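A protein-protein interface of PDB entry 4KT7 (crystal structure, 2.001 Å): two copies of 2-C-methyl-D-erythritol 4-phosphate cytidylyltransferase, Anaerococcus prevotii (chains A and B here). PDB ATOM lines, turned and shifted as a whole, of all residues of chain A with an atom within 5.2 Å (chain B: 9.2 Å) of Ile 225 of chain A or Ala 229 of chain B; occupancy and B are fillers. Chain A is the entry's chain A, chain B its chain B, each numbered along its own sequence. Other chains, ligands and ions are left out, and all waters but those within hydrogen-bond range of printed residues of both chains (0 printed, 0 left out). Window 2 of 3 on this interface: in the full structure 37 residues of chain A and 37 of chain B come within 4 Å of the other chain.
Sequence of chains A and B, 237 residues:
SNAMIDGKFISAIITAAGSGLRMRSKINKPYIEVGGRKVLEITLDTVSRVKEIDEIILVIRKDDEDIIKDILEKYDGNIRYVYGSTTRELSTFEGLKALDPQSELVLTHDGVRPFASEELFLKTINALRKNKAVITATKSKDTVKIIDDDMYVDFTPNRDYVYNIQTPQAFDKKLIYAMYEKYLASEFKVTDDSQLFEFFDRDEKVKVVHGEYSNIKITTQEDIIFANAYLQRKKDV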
ATOM      1  N   GLN A 221      15.699  26.630 -18.380  1.00  0.00           N
ATOM      2  CA  GLN A 221      15.560  25.364 -19.087  1.00  0.00           C
ATOM      3  C   GLN A 221      14.887  24.322 -18.191  1.00  0.00           C
ATOM      4  O   GLN A 221      14.116  23.484 -18.665  1.00  0.00           O
ATOM      5  CB  GLN A 221      16.922  24.870 -19.576  1.00  0.00           C
ATOM      6  CG  GLN A 221      16.843  23.684 -20.525  1.00  0.00           C
ATOM      7  CD  GLN A 221      15.796  23.876 -21.613  1.00  0.00           C
ATOM      8  OE1 GLN A 221      15.767  24.907 -22.286  1.00  0.00           O
ATOM      9  NE2 GLN A 221      14.923  22.883 -21.781  1.00  0.00           N
ATOM     10  N   GLU A 222      15.168  24.397 -16.891  1.00  0.00           N
ATOM     11  CA  GLU A 222      14.540  23.516 -15.906  1.00  0.00           C
ATOM     12  C   GLU A 222      13.020  23.691 -15.852  1.00  0.00           C
ATOM     13  O   GLU A 222      12.288  22.701 -15.790  1.00  0.00           O
ATOM     14  CB  GLU A 222      15.147  23.727 -14.509  1.00  0.00           C
ATOM     15  CG  GLU A 222      16.473  23.007 -14.268  1.00  0.00           C
ATOM     16  CD  GLU A 222      17.682  23.890 -14.521  1.00  0.00           C
ATOM     17  OE1 GLU A 222      17.500  25.098 -14.795  1.00  0.00           O
ATOM     18  OE2 GLU A 222      18.819  23.373 -14.443  1.00  0.00           O
ATOM     19  N   ASP A 223      12.556  24.944 -15.870  1.00  0.00           N
ATOM     20  CA  ASP A 223      11.121  25.254 -15.833  1.00  0.00           C
ATOM     21  C   ASP A 223      10.396  24.657 -17.039  1.00  0.00           C
ATOM     22  O   ASP A 223       9.302  24.118 -16.906  1.00  0.00           O
ATOM     23  CB  ASP A 223      10.884  26.770 -15.788  1.00  0.00           C
ATOM     24  CG  ASP A 223      11.383  27.409 -14.501  1.00  0.00           C
ATOM     25  OD1 ASP A 223      11.361  26.736 -13.452  1.00  0.00           O
ATOM     26  OD2 ASP A 223      11.790  28.590 -14.539  1.00  0.00           O
ATOM     27  N   ILE A 224      11.024  24.741 -18.211  1.00  0.00           N
ATOM     28  CA  ILE A 224      10.453  24.194 -19.440  1.00  0.00           C
ATOM     29  C   ILE A 224      10.290  22.674 -19.352  1.00  0.00           C
ATOM     30  O   ILE A 224       9.226  22.133 -19.676  1.00  0.00           O
ATOM     31  CB  ILE A 224      11.303  24.591 -20.663  1.00  0.00           C
ATOM     32  CG1 ILE A 224      11.152  26.093 -20.910  1.00  0.00           C
ATOM     33  CG2 ILE A 224      10.890  23.801 -21.897  1.00  0.00           C
ATOM     34  CD1 ILE A 224      12.124  26.644 -21.910  1.00  0.00           C
ATOM     35  N   ILE A 225      11.344  21.998 -18.898  1.00  0.00           N
ATOM     36  CA  ILE A 225      11.278  20.572 -18.599  1.00  0.00           C
ATOM     37  C   ILE A 225      10.116  20.298 -17.636  1.00  0.00           C
ATOM     38  O   ILE A 225       9.328  19.381 -17.850  1.00  0.00           O
ATOM     39  CB  ILE A 225      12.612  20.054 -17.986  1.00  0.00           C
ATOM     40  CG1 ILE A 225      13.793  20.316 -18.930  1.00  0.00           C
ATOM     41  CG2 ILE A 225      12.528  18.571 -17.647  1.00  0.00           C
ATOM     42  CD1 ILE A 225      13.577  19.840 -20.355  1.00  0.00           C
ATOM     43  N   PHE A 226       9.995  21.115 -16.593  1.00  0.00           N
ATOM     44  CA  PHE A 226       8.954  20.918 -15.594  1.00  0.00           C
ATOM     45  C   PHE A 226       7.565  21.200 -16.177  1.00  0.00           C
ATOM     46  O   PHE A 226       6.604  20.477 -15.899  1.00  0.00           O
ATOM     47  CB  PHE A 226       9.220  21.807 -14.369  1.00  0.00           C
ATOM     48  CG  PHE A 226       8.616  21.283 -13.094  1.00  0.00           C
ATOM     49  CD1 PHE A 226       9.288  20.333 -12.335  1.00  0.00           C
ATOM     50  CD2 PHE A 226       7.381  21.737 -12.652  1.00  0.00           C
ATOM     51  CE1 PHE A 226       8.736  19.837 -11.162  1.00  0.00           C
ATOM     52  CE2 PHE A 226       6.824  21.247 -11.477  1.00  0.00           C
ATOM     53  CZ  PHE A 226       7.503  20.298 -10.731  1.00  0.00           C
ATOM     54  N   ALA A 227       7.460  22.251 -16.987  1.00  0.00           N
ATOM     55  CA  ALA A 227       6.174  22.616 -17.579  1.00  0.00           C
ATOM     56  C   ALA A 227       5.687  21.513 -18.505  1.00  0.00           C
ATOM     57  O   ALA A 227       4.525  21.139 -18.459  1.00  0.00           O
ATOM     58  CB  ALA A 227       6.269  23.932 -18.324  1.00  0.00           C
ATOM     59  N   ASN A 228       6.577  20.987 -19.339  1.00  0.00           N
ATOM     60  CA  ASN A 228       6.215  19.878 -20.222  1.00  0.00           C
ATOM     61  C   ASN A 228       5.748  18.612 -19.486  1.00  0.00           C
ATOM     62  O   ASN A 228       4.822  17.935 -19.941  1.00  0.00           O
ATOM     63  CB  ASN A 228       7.358  19.555 -21.191  1.00  0.00           C
ATOM     64  CG  ASN A 228       7.451  20.546 -22.336  1.00  0.00           C
ATOM     65  OD1 ASN A 228       6.440  21.098 -22.785  1.00  0.00           O
ATOM     66  ND2 ASN A 228       8.666  20.771 -22.822  1.00  0.00           N
ATOM     67  N   ALA A 229       6.381  18.296 -18.355  1.00  0.00           N
ATOM     68  CA  ALA A 229       5.986  17.125 -17.561  1.00  0.00           C
ATOM     69  C   ALA A 229       4.613  17.328 -16.916  1.00  0.00           C
ATOM     70  O   ALA A 229       3.852  16.374 -16.765  1.00  0.00           O
ATOM     71  CB  ALA A 229       7.042  16.789 -16.506  1.00  0.00           C
ATOM     72  N   VAL B  34      14.717   6.531 -10.752  1.00  0.00           N
ATOM     73  CA  VAL B  34      15.209   7.483 -11.742  1.00  0.00           C
ATOM     74  C   VAL B  34      16.582   7.066 -12.275  1.00  0.00           C
ATOM     75  O   VAL B  34      17.441   6.591 -11.521  1.00  0.00           O
ATOM     76  CB  VAL B  34      15.264   8.921 -11.169  1.00  0.00           C
ATOM     77  CG1 VAL B  34      13.867   9.399 -10.817  1.00  0.00           C
ATOM     78  CG2 VAL B  34      16.146   8.974  -9.940  1.00  0.00           C
ATOM     79  N   GLY B  35      16.776   7.228 -13.579  1.00  0.00           N
ATOM     80  CA  GLY B  35      18.016   6.829 -14.216  1.00  0.00           C
ATOM     81  C   GLY B  35      18.275   5.345 -14.045  1.00  0.00           C
ATOM     82  O   GLY B  35      19.430   4.918 -13.984  1.00  0.00           O
ATOM     83  N   PHE B 115      19.719  13.871  -4.762  1.00  0.00           N
ATOM     84  CA  PHE B 115      20.714  14.719  -5.436  1.00  0.00           C
ATOM     85  C   PHE B 115      21.620  15.544  -4.518  1.00  0.00           C
ATOM     86  O   PHE B 115      22.480  16.283  -5.002  1.00  0.00           O
ATOM     87  CB  PHE B 115      20.031  15.629  -6.464  1.00  0.00           C
ATOM     88  CG  PHE B 115      19.226  14.867  -7.487  1.00  0.00           C
ATOM     89  CD1 PHE B 115      19.736  13.712  -8.063  1.00  0.00           C
ATOM     90  CD2 PHE B 115      17.956  15.281  -7.841  1.00  0.00           C
ATOM     91  CE1 PHE B 115      18.996  12.998  -8.996  1.00  0.00           C
ATOM     92  CE2 PHE B 115      17.211  14.570  -8.767  1.00  0.00           C
ATOM     93  CZ  PHE B 115      17.740  13.429  -9.350  1.00  0.00           C
ATOM     94  N   ILE B 218      11.761  13.949  -4.337  1.00  0.00           N
ATOM     95  CA  ILE B 218      11.125  13.267  -5.459  1.00  0.00           C
ATOM     96  C   ILE B 218       9.957  12.437  -4.958  1.00  0.00           C
ATOM     97  O   ILE B 218      10.144  11.350  -4.411  1.00  0.00           O
ATOM     98  CB  ILE B 218      12.135  12.423  -6.266  1.00  0.00           C
ATOM     99  CG1 ILE B 218      13.195  13.352  -6.866  1.00  0.00           C
ATOM    100  CG2 ILE B 218      11.439  11.632  -7.372  1.00  0.00           C
ATOM    101  CD1 ILE B 218      14.324  12.639  -7.528  1.00  0.00           C
ATOM    102  N   GLU B 222       5.905  13.837 -11.788  1.00  0.00           N
ATOM    103  CA  GLU B 222       6.602  14.812 -12.618  1.00  0.00           C
ATOM    104  C   GLU B 222       8.033  15.031 -12.143  1.00  0.00           C
ATOM    105  O   GLU B 222       8.937  15.247 -12.960  1.00  0.00           O
ATOM    106  CB  GLU B 222       5.830  16.135 -12.655  1.00  0.00           C
ATOM    107  CG  GLU B 222       4.399  16.017 -13.176  1.00  0.00           C
ATOM    108  CD  GLU B 222       3.419  15.527 -12.120  1.00  0.00           C
ATOM    109  OE1 GLU B 222       3.696  14.497 -11.466  1.00  0.00           O
ATOM    110  OE2 GLU B 222       2.368  16.178 -11.942  1.00  0.00           O
ATOM    111  N   ASP B 223       8.227  14.983 -10.824  1.00  0.00           N
ATOM    112  CA  ASP B 223       9.560  15.017 -10.227  1.00  0.00           C
ATOM    113  C   ASP B 223      10.445  13.931 -10.847  1.00  0.00           C
ATOM    114  O   ASP B 223      11.593  14.187 -11.209  1.00  0.00           O
ATOM    115  CB  ASP B 223       9.482  14.804  -8.710  1.00  0.00           C
ATOM    116  CG  ASP B 223       8.651  15.866  -8.000  1.00  0.00           C
ATOM    117  OD1 ASP B 223       8.498  16.981  -8.540  1.00  0.00           O
ATOM    118  OD2 ASP B 223       8.158  15.585  -6.888  1.00  0.00           O
ATOM    119  N   ILE B 224       9.897  12.723 -10.968  1.00  0.00           N
ATOM    120  CA  ILE B 224      10.584  11.596 -11.606  1.00  0.00           C
ATOM    121  C   ILE B 224      11.066  11.938 -13.020  1.00  0.00           C
ATOM    122  O   ILE B 224      12.243  11.741 -13.348  1.00  0.00           O
ATOM    123  CB  ILE B 224       9.671  10.350 -11.685  1.00  0.00           C
ATOM    124  CG1 ILE B 224       9.229   9.912 -10.286  1.00  0.00           C
ATOM    125  CG2 ILE B 224      10.376   9.209 -12.408  1.00  0.00           C
ATOM    126  CD1 ILE B 224       8.269   8.727 -10.302  1.00  0.00           C
ATOM    127  N   ILE B 225      10.157  12.437 -13.855  1.00  0.00           N
ATOM    128  CA  ILE B 225      10.519  12.911 -15.189  1.00  0.00           C
ATOM    129  C   ILE B 225      11.593  13.994 -15.119  1.00  0.00           C
ATOM    130  O   ILE B 225      12.613  13.910 -15.804  1.00  0.00           O
ATOM    131  CB  ILE B 225       9.300  13.469 -15.943  1.00  0.00           C
ATOM    132  CG1 ILE B 225       8.243  12.372 -16.136  1.00  0.00           C
ATOM    133  CG2 ILE B 225       9.735  14.046 -17.281  1.00  0.00           C
ATOM    134  CD1 ILE B 225       6.830  12.898 -16.256  1.00  0.00           C
ATOM    135  N   PHE B 226      11.363  15.006 -14.284  1.00  0.00           N
ATOM    136  CA  PHE B 226      12.333  16.074 -14.098  1.00  0.00           C
ATOM    137  C   PHE B 226      13.675  15.482 -13.654  1.00  0.00           C
ATOM    138  O   PHE B 226      14.734  15.894 -14.132  1.00  0.00           O
ATOM    139  CB  PHE B 226      11.818  17.079 -13.062  1.00  0.00           C
ATOM    140  CG  PHE B 226      12.803  18.162 -12.720  1.00  0.00           C
ATOM    141  CD1 PHE B 226      13.765  17.964 -11.738  1.00  0.00           C
ATOM    142  CD2 PHE B 226      12.758  19.388 -13.368  1.00  0.00           C
ATOM    143  CE1 PHE B 226      14.676  18.965 -11.422  1.00  0.00           C
ATOM    144  CE2 PHE B 226      13.662  20.395 -13.051  1.00  0.00           C
ATOM    145  CZ  PHE B 226      14.625  20.182 -12.077  1.00  0.00           C
ATOM    146  N   ALA B 227      13.616  14.511 -12.745  1.00  0.00           N
ATOM    147  CA  ALA B 227      14.821  13.891 -12.194  1.00  0.00           C
ATOM    148  C   ALA B 227      15.611  13.095 -13.235  1.00  0.00           C
ATOM    149  O   ALA B 227      16.847  13.058 -13.188  1.00  0.00           O
ATOM    150  CB  ALA B 227      14.467  13.006 -11.018  1.00  0.00           C
ATOM    151  N   ASN B 228      14.901  12.446 -14.157  1.00  0.00           N
ATOM    152  CA  ASN B 228      15.552  11.713 -15.239  1.00  0.00           C
ATOM    153  C   ASN B 228      16.293  12.665 -16.172  1.00  0.00           C
ATOM    154  O   ASN B 228      17.360  12.332 -16.690  1.00  0.00           O
ATOM    155  CB  ASN B 228      14.542  10.873 -16.026  1.00  0.00           C
ATOM    156  CG  ASN B 228      14.067   9.658 -15.253  1.00  0.00           C
ATOM    157  OD1 ASN B 228      14.835   8.726 -15.004  1.00  0.00           O
ATOM    158  ND2 ASN B 228      12.792   9.656 -14.880  1.00  0.00           N
ATOM    159  N   ALA B 229      15.728  13.853 -16.375  1.00  0.00           N
ATOM    160  CA  ALA B 229      16.348  14.847 -17.244  1.00  0.00           C
ATOM    161  C   ALA B 229      17.570  15.479 -16.570  1.00  0.00           C
ATOM    162  O   ALA B 229      18.605  15.678 -17.209  1.00  0.00           O
ATOM    163  CB  ALA B 229      15.343  15.909 -17.646  1.00  0.00           C
ATOM    164  N   TYR B 230      17.448  15.786 -15.282  1.00  0.00           N
ATOM    165  CA  TYR B 230      18.562  16.351 -14.524  1.00  0.00           C
ATOM    166  C   TYR B 230      19.812  15.445 -14.564  1.00  0.00           C
ATOM    167  O   TYR B 230      20.918  15.935 -14.794  1.00  0.00           O
ATOM    168  CB  TYR B 230      18.123  16.679 -13.088  1.00  0.00           C
ATOM    169  CG  TYR B 230      19.237  17.098 -12.162  1.00  0.00           C
ATOM    170  CD1 TYR B 230      19.737  18.398 -12.178  1.00  0.00           C
ATOM    171  CD2 TYR B 230      19.778  16.201 -11.253  1.00  0.00           C
ATOM    172  CE1 TYR B 230      20.763  18.781 -11.324  1.00  0.00           C
ATOM    173  CE2 TYR B 230      20.800  16.578 -10.392  1.00  0.00           C
ATOM    174  CZ  TYR B 230      21.288  17.866 -10.434  1.00  0.00           C
ATOM    175  OH  TYR B 230      22.303  18.231  -9.580  1.00  0.00           O
ATOM    176  N   LEU B 231      19.642  14.134 -14.372  1.00  0.00           N
ATOM    177  CA  LEU B 231      20.762  13.179 -14.502  1.00  0.00           C
ATOM    178  C   LEU B 231      21.441  13.240 -15.877  1.00  0.00           C
ATOM    179  O   LEU B 231      22.664  13.145 -15.982  1.00  0.00           O
ATOM    180  CB  LEU B 231      20.317  11.735 -14.200  1.00  0.00           C
ATOM    181  CG  LEU B 231      19.997  11.314 -12.756  1.00  0.00           C
ATOM    182  CD1 LEU B 231      19.532   9.868 -12.699  1.00  0.00           C
ATOM    183  CD2 LEU B 231      21.195  11.510 -11.839  1.00  0.00           C
ATOM    184  N   GLN B 232      20.643  13.415 -16.925  1.00  0.00           N
ATOM    185  CA  GLN B 232      21.162  13.462 -18.291  1.00  0.00           C
ATOM    186  C   GLN B 232      21.978  14.731 -18.595  1.00  0.00           C
ATOM    187  O   GLN B 232      22.800  14.740 -19.514  1.00  0.00           O
ATOM    188  CB  GLN B 232      20.018  13.298 -19.294  1.00  0.00           C
ATOM    189  CG  GLN B 232      19.269  11.975 -19.171  1.00  0.00           C
ATOM    190  CD  GLN B 232      18.234  11.807 -20.260  1.00  0.00           C
ATOM    191  OE1 GLN B 232      17.863  12.773 -20.927  1.00  0.00           O
ATOM    192  NE2 GLN B 232      17.767  10.577 -20.457  1.00  0.00           N
ATOM    193  N   ARG B 233      21.744  15.795 -17.830  1.00  0.00           N
ATOM    194  CA  ARG B 233      22.560  17.003 -17.936  1.00  0.00           C
ATOM    195  C   ARG B 233      23.690  16.967 -16.916  1.00  0.00           C
ATOM    196  O   ARG B 233      24.818  17.346 -17.218  1.00  0.00           O
ATOM    197  CB  ARG B 233      21.715  18.260 -17.718  1.00  0.00           C
ATOM    198  CG  ARG B 233      20.891  18.694 -18.925  1.00  0.00           C
ATOM    199  CD  ARG B 233      20.204  20.034 -18.671  1.00  0.00           C
ATOM    200  NE  ARG B 233      19.337  19.998 -17.493  1.00  0.00           N
ATOM    201  CZ  ARG B 233      19.676  20.463 -16.294  1.00  0.00           C
ATOM    202  NH1 ARG B 233      20.871  21.006 -16.106  1.00  0.00           N
ATOM    203  NH2 ARG B 233      18.821  20.384 -15.282  1.00  0.00           N
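OE2 of Glu 222 of chain A lies within salt-bridge range of NH2 of Arg 233 of chain B (3.1 Å).
Printed residues of chain B that touch a printed residue of chain A: Glu 222, Asp 223, Ile 225, Phe 226, Ala 229 and Arg 233. Along chain B the printed residues that touch a printed residue of chain A span positions 222 to 233. Of the 9 printed residues of chain A, 4 touch a printed residue of chain B. Hydrophobic or aromatic side chains of chain A within 4 Å of the printed part of chain B: Ile 225, Phe 226 and Ala 229.
Asp 223 of chain A touches none of the printed residues of chain B. Of the printed residues of chain B, Ile 225 of chain A touches Ala 229. Of the printed residues of chain A, Glu 222 of chain B touches Ala 229 (3.6 Å). Printed residues of chain A within 4 Å of Asp 223 of chain B: Phe 226. Of the printed residues of chain A, Phe 226 of chain B touches Glu 222 and Phe 226. Of the printed residues of chain A, Ala 229 of chain B touches Ile 225. The nearest printed residue of chain A that does not touch Ala 229 of chain B is Phe 226 of chain A (7.5 Å).
Glu 222 of chain A touches Phe 226 of chain B, but with the chains exchanged Phe 226 of chain A does not touch Glu 222 of chain B (4.9 Å). Phe 226 of chain A touches Asp 223 of chain B, but with the chains exchanged Asp 223 of chain A does not touch Phe 226 of chain B (5.5 Å). Phe 226 of chain B touches its own counterpart, Phe 226 of chain A. Ala 229 of chain A touches Glu 222 of chain B, but with the chains exchanged Glu 222 of chain A does not touch Ala 229 of chain B (7.7 Å). Positions printed for both chains: 222, 223, 224, 225, 226, 227, 228 and 229. Of the 7 pairs that touch across the chains among the printed residues, 3 have their exchanged pair printed and touching as well.
Among the printed residues, merely in contact across the chains: Glu 222 of chain A with Phe 226 of chain B (3.8 Å), Ile 225 of chain A with Ala 229 of chain B (3.9 Å), Phe 226 of chain A with Asp 223 of chain B (3.9 Å), Phe 226 of chain A with Phe 226 of chain B (3.7 Å), Ala 229 of chain A with Glu 222 of chain B (3.6 Å) and Ala 229 of chain A with Ile 225 of chain B (3.9 Å).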
